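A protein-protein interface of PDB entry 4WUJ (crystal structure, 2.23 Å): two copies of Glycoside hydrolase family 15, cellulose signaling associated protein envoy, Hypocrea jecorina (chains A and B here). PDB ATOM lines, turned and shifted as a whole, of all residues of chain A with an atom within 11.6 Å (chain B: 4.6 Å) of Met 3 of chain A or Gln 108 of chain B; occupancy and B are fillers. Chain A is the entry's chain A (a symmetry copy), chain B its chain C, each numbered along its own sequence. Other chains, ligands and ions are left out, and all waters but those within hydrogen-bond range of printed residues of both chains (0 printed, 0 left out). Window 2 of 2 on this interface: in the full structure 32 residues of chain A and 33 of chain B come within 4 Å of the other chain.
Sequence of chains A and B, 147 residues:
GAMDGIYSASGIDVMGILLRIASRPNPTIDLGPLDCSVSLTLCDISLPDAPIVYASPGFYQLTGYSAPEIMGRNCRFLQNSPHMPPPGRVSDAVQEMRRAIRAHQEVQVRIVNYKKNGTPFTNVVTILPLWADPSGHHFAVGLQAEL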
ATOM      1  N   GLY A   1     -25.070  -5.673 -15.294  1.00  0.00           N
ATOM      2  CA  GLY A   1     -23.952  -5.144 -16.062  1.00  0.00           C
ATOM      3  C   GLY A   1     -22.676  -5.905 -15.779  1.00  0.00           C
ATOM      4  O   GLY A   1     -21.689  -5.753 -16.489  1.00  0.00           O
ATOM      5  N   ALA A   2     -22.692  -6.784 -14.785  1.00  0.00           N
ATOM      6  CA  ALA A   2     -21.482  -7.507 -14.475  1.00  0.00           C
ATOM      7  C   ALA A   2     -21.162  -8.498 -15.629  1.00  0.00           C
ATOM      8  O   ALA A   2     -20.089  -9.056 -15.670  1.00  0.00           O
ATOM      9  CB  ALA A   2     -21.630  -8.230 -13.203  1.00  0.00           C
ATOM     10  N   MET A   3     -22.099  -8.728 -16.542  1.00  0.00           N
ATOM     11  CA  MET A   3     -21.857  -9.673 -17.657  1.00  0.00           C
ATOM     12  C   MET A   3     -21.440  -8.966 -18.968  1.00  0.00           C
ATOM     13  O   MET A   3     -21.288  -9.618 -19.985  1.00  0.00           O
ATOM     14  CB  MET A   3     -23.089 -10.544 -17.914  1.00  0.00           C
ATOM     15  CG  MET A   3     -23.494 -11.449 -16.716  1.00  0.00           C
ATOM     16  SD  MET A   3     -25.055 -12.333 -16.973  1.00  0.00           S
ATOM     17  CE  MET A   3     -26.297 -11.051 -17.208  1.00  0.00           C
ATOM     18  N   ASP A   4     -21.275  -7.645 -18.928  1.00  0.00           N
ATOM     19  CA  ASP A   4     -20.851  -6.857 -20.095  1.00  0.00           C
ATOM     20  C   ASP A   4     -19.552  -7.483 -20.646  1.00  0.00           C
ATOM     21  O   ASP A   4     -18.595  -7.610 -19.896  1.00  0.00           O
ATOM     22  CB  ASP A   4     -20.587  -5.374 -19.682  1.00  0.00           C
ATOM     23  CG  ASP A   4     -21.900  -4.545 -19.413  1.00  0.00           C
ATOM     24  OD1 ASP A   4     -23.001  -5.059 -19.704  1.00  0.00           O
ATOM     25  OD2 ASP A   4     -21.827  -3.360 -18.928  1.00  0.00           O
ATOM     26  N   GLY A   5     -19.529  -7.939 -21.903  1.00  0.00           N
ATOM     27  CA  GLY A   5     -18.268  -8.370 -22.569  1.00  0.00           C
ATOM     28  C   GLY A   5     -17.617  -9.667 -22.082  1.00  0.00           C
ATOM     29  O   GLY A   5     -16.501 -10.015 -22.483  1.00  0.00           O
ATOM     30  N   ILE A   6     -18.316 -10.443 -21.250  1.00  0.00           N
ATOM     31  CA  ILE A   6     -17.722 -11.688 -20.738  1.00  0.00           C
ATOM     32  C   ILE A   6     -17.452 -12.730 -21.833  1.00  0.00           C
ATOM     33  O   ILE A   6     -16.709 -13.687 -21.634  1.00  0.00           O
ATOM     34  CB  ILE A   6     -18.601 -12.320 -19.624  1.00  0.00           C
ATOM     35  CG1 ILE A   6     -19.884 -12.894 -20.222  1.00  0.00           C
ATOM     36  CG2 ILE A   6     -18.876 -11.274 -18.546  1.00  0.00           C
ATOM     37  CD1 ILE A   6     -20.647 -13.828 -19.255  1.00  0.00           C
ATOM     38  N   TYR A   7     -18.081 -12.548 -22.982  1.00  0.00           N
ATOM     39  CA  TYR A   7     -17.845 -13.481 -24.083  1.00  0.00           C
ATOM     40  C   TYR A   7     -16.796 -12.914 -25.095  1.00  0.00           C
ATOM     41  O   TYR A   7     -16.607 -13.493 -26.157  1.00  0.00           O
ATOM     42  CB  TYR A   7     -19.149 -13.887 -24.785  1.00  0.00           C
ATOM     43  CG  TYR A   7     -20.142 -14.642 -23.901  1.00  0.00           C
ATOM     44  CD1 TYR A   7     -19.745 -15.729 -23.123  1.00  0.00           C
ATOM     45  CD2 TYR A   7     -21.480 -14.248 -23.848  1.00  0.00           C
ATOM     46  CE1 TYR A   7     -20.693 -16.431 -22.275  1.00  0.00           C
ATOM     47  CE2 TYR A   7     -22.447 -14.956 -23.020  1.00  0.00           C
ATOM     48  CZ  TYR A   7     -22.040 -16.036 -22.250  1.00  0.00           C
ATOM     49  OH  TYR A   7     -22.987 -16.687 -21.450  1.00  0.00           O
ATOM     50  N   SER A   8     -16.117 -11.807 -24.744  1.00  0.00           N
ATOM     51  CA  SER A   8     -14.848 -11.456 -25.411  1.00  0.00           C
ATOM     52  C   SER A   8     -13.806 -11.060 -24.365  1.00  0.00           C
ATOM     53  O   SER A   8     -13.832  -9.949 -23.833  1.00  0.00           O
ATOM     54  CB  SER A   8     -15.093 -10.368 -26.471  1.00  0.00           C
ATOM     55  OG  SER A   8     -13.904  -9.764 -26.932  1.00  0.00           O
ATOM     56  N   ALA A   9     -12.926 -11.996 -24.028  1.00  0.00           N
ATOM     57  CA  ALA A   9     -11.785 -11.722 -23.155  1.00  0.00           C
ATOM     58  C   ALA A   9     -10.922 -10.528 -23.666  1.00  0.00           C
ATOM     59  O   ALA A   9     -10.370  -9.753 -22.887  1.00  0.00           O
ATOM     60  CB  ALA A   9     -10.914 -12.983 -23.056  1.00  0.00           C
ATOM     61  N   GLY A  11     -12.084  -8.032 -25.251  1.00  0.00           N
ATOM     62  CA  GLY A  11     -12.955  -6.887 -25.481  1.00  0.00           C
ATOM     63  C   GLY A  11     -13.073  -6.494 -26.961  1.00  0.00           C
ATOM     64  O   GLY A  11     -13.690  -5.485 -27.329  1.00  0.00           O
ATOM     65  N   ILE B  29     -31.655 -11.738 -24.701  1.00  0.00           N
ATOM     66  CA  ILE B  29     -30.402 -11.472 -24.023  1.00  0.00           C
ATOM     67  C   ILE B  29     -29.545 -10.716 -24.998  1.00  0.00           C
ATOM     68  O   ILE B  29     -29.628 -10.953 -26.202  1.00  0.00           O
ATOM     69  CB  ILE B  29     -29.677 -12.758 -23.641  1.00  0.00           C
ATOM     70  CG1 ILE B  29     -30.483 -13.520 -22.594  1.00  0.00           C
ATOM     71  CG2 ILE B  29     -28.269 -12.460 -23.146  1.00  0.00           C
ATOM     72  CD1 ILE B  29     -31.232 -14.699 -23.197  1.00  0.00           C
ATOM     73  N   GLU B  96     -34.328 -24.394 -15.441  1.00  0.00           N
ATOM     74  CA  GLU B  96     -34.493 -23.262 -16.357  1.00  0.00           C
ATOM     75  C   GLU B  96     -33.844 -23.642 -17.708  1.00  0.00           C
ATOM     76  O   GLU B  96     -34.467 -23.500 -18.755  1.00  0.00           O
ATOM     77  CB  GLU B  96     -33.875 -21.991 -15.765  1.00  0.00           C
ATOM     78  CG  GLU B  96     -34.642 -20.706 -16.106  1.00  0.00           C
ATOM     79  CD  GLU B  96     -33.867 -19.409 -15.772  1.00  0.00           C
ATOM     80  OE1 GLU B  96     -33.031 -19.392 -14.829  1.00  0.00           O
ATOM     81  OE2 GLU B  96     -34.094 -18.405 -16.483  1.00  0.00           O
ATOM     82  N   GLU B 106     -34.365 -18.904 -25.891  1.00  0.00           N
ATOM     83  CA  GLU B 106     -33.130 -18.330 -25.384  1.00  0.00           C
ATOM     84  C   GLU B 106     -33.192 -18.403 -23.895  1.00  0.00           C
ATOM     85  O   GLU B 106     -34.267 -18.241 -23.326  1.00  0.00           O
ATOM     86  CB  GLU B 106     -33.028 -16.850 -25.759  1.00  0.00           C
ATOM     87  CG  GLU B 106     -32.709 -16.614 -27.201  1.00  0.00           C
ATOM     88  CD  GLU B 106     -32.910 -15.167 -27.615  1.00  0.00           C
ATOM     89  OE1 GLU B 106     -32.477 -14.243 -26.865  1.00  0.00           O
ATOM     90  OE2 GLU B 106     -33.491 -14.978 -28.712  1.00  0.00           O
ATOM     91  N   VAL B 107     -32.043 -18.574 -23.259  1.00  0.00           N
ATOM     92  CA  VAL B 107     -31.990 -18.568 -21.831  1.00  0.00           C
ATOM     93  C   VAL B 107     -30.611 -18.245 -21.381  1.00  0.00           C
ATOM     94  O   VAL B 107     -29.615 -18.613 -22.012  1.00  0.00           O
ATOM     95  CB  VAL B 107     -32.381 -19.946 -21.253  1.00  0.00           C
ATOM     96  CG1 VAL B 107     -31.501 -21.048 -21.856  1.00  0.00           C
ATOM     97  CG2 VAL B 107     -32.280 -19.953 -19.746  1.00  0.00           C
ATOM     98  N   GLN B 108     -30.531 -17.550 -20.268  1.00  0.00           N
ATOM     99  CA  GLN B 108     -29.235 -17.253 -19.712  1.00  0.00           C
ATOM    100  C   GLN B 108     -29.334 -17.380 -18.223  1.00  0.00           C
ATOM    101  O   GLN B 108     -30.173 -16.725 -17.580  1.00  0.00           O
ATOM    102  CB  GLN B 108     -28.753 -15.859 -20.142  1.00  0.00           C
ATOM    103  CG  GLN B 108     -27.455 -15.438 -19.507  1.00  0.00           C
ATOM    104  CD  GLN B 108     -26.993 -14.060 -19.992  1.00  0.00           C
ATOM    105  OE1 GLN B 108     -27.659 -13.046 -19.768  1.00  0.00           O
ATOM    106  NE2 GLN B 108     -25.871 -14.031 -20.692  1.00  0.00           N
ATOM    107  N   VAL B 109     -28.475 -18.232 -17.685  1.00  0.00           N
ATOM    108  CA  VAL B 109     -28.414 -18.476 -16.272  1.00  0.00           C
ATOM    109  C   VAL B 109     -26.973 -18.524 -15.847  1.00  0.00           C
ATOM    110  O   VAL B 109     -26.054 -18.549 -16.653  1.00  0.00           O
ATOM    111  CB  VAL B 109     -29.045 -19.861 -15.888  1.00  0.00           C
ATOM    112  CG1 VAL B 109     -30.353 -20.083 -16.631  1.00  0.00           C
ATOM    113  CG2 VAL B 109     -28.062 -20.993 -16.163  1.00  0.00           C
ATOM    114  N   VAL B 124     -21.229 -18.465 -16.676  1.00  0.00           N
ATOM    115  CA  VAL B 124     -22.399 -17.772 -17.232  1.00  0.00           C
ATOM    116  C   VAL B 124     -22.744 -18.359 -18.617  1.00  0.00           C
ATOM    117  O   VAL B 124     -22.138 -18.023 -19.670  1.00  0.00           O
ATOM    118  CB  VAL B 124     -22.256 -16.252 -17.271  1.00  0.00           C
ATOM    119  CG1 VAL B 124     -23.538 -15.598 -17.749  1.00  0.00           C
ATOM    120  CG2 VAL B 124     -21.838 -15.709 -15.891  1.00  0.00           C
ATOM    121  N   VAL B 125     -23.745 -19.237 -18.581  1.00  0.00           N
ATOM    122  CA  VAL B 125     -24.147 -20.028 -19.733  1.00  0.00           C
ATOM    123  C   VAL B 125     -25.318 -19.397 -20.389  1.00  0.00           C
ATOM    124  O   VAL B 125     -26.322 -19.072 -19.742  1.00  0.00           O
ATOM    125  CB  VAL B 125     -24.566 -21.453 -19.316  1.00  0.00           C
ATOM    126  CG1 VAL B 125     -24.973 -22.241 -20.520  1.00  0.00           C
ATOM    127  CG2 VAL B 125     -23.428 -22.172 -18.571  1.00  0.00           C
ATOM    128  N   THR B 126     -25.217 -19.237 -21.686  1.00  0.00           N
ATOM    129  CA  THR B 126     -26.340 -18.769 -22.501  1.00  0.00           C
ATOM    130  C   THR B 126     -26.627 -19.813 -23.563  1.00  0.00           C
ATOM    131  O   THR B 126     -25.711 -20.238 -24.262  1.00  0.00           O
ATOM    132  CB  THR B 126     -25.983 -17.492 -23.294  1.00  0.00           C
ATOM    133  OG1 THR B 126     -25.550 -16.476 -22.403  1.00  0.00           O
ATOM    134  CG2 THR B 126     -27.178 -17.006 -24.103  1.00  0.00           C
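The backbone carbonyl oxygen (O) of Val 124 of chain B sits close to the side-chain hydroxyl (OH) of Tyr 7 of chain A (2.4 Å). OG1 of Thr 126 of chain B lies within hydrogen-bond range of OH of Tyr 7 of chain A, at 2.7 Å.
The backbone carbonyl oxygen of Val 109 of chain B sits at hydrogen-bond distance from the backbone NH of Val 125 of chain B, 3.1 Å away. The side-chain hydroxyl (OG1) of Thr 126 of chain B lies within hydrogen-bond range of the side-chain amide nitrogen (NE2) of Gln 108 of chain B (3.0 Å).
CE of Met 3 of chain A touches OE1 of Gln 108 of chain B, 3.5 Å away. Met 3 of chain A touches Val 124 of chain B. Val 124 of chain B touches Ile 6 of chain A (CB to CD1, 3.5 Å). NE2 of Gln 108 of chain B touches OH of Tyr 7 of chain A (3.99 Å). Tyr 7 of chain A touches Val 125 of chain B.
Gly 1 of chain A touches none of the printed residues of chain B. Of the printed residues of chain B, Ile 6 of chain A touches Val 124. Printed residues of chain B within 4 Å of Tyr 7 of chain A: Gln 108 (3.99 Å), Val 124 (2.4 Å), Val 125 (3.7 Å) and Thr 126 (2.7 Å). No residue of chain A comes within 4 Å of Ile 29 of chain B. Glu 96 of chain B touches none of the printed residues of chain A. No residue of chain A comes within 4 Å of Val 107 of chain B. Of the printed residues of chain A, Gln 108 of chain B touches Met 3 (3.5 Å) and Tyr 7 (3.99 Å). No residue of chain A comes within 4 Å of Val 109 of chain B. Of chain A, only Met 3 (3.7 Å), Ile 6 (3.5 Å) and Tyr 7 (2.4 Å) come within 4 Å of Val 124 of chain B. Of the printed residues of chain A, Val 125 of chain B touches Tyr 7. The nearest printed residue of chain B that does not touch Met 3 of chain A is Val 109 of chain B (6.3 Å).
Of the 10 printed residues of chain A, 3 touch a printed residue of chain B. Hydrophobic or aromatic side chains of chain A within 4 Å of the printed part of chain B: Met 3, Ile 6 and Tyr 7. Among the printed residues, 7 pairs touch across the chains. Among the printed residues, no Asp or Glu carboxylate lies within 4 Å of a Lys or Arg side-chain nitrogen of the other chain.
No position is printed for both chains.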
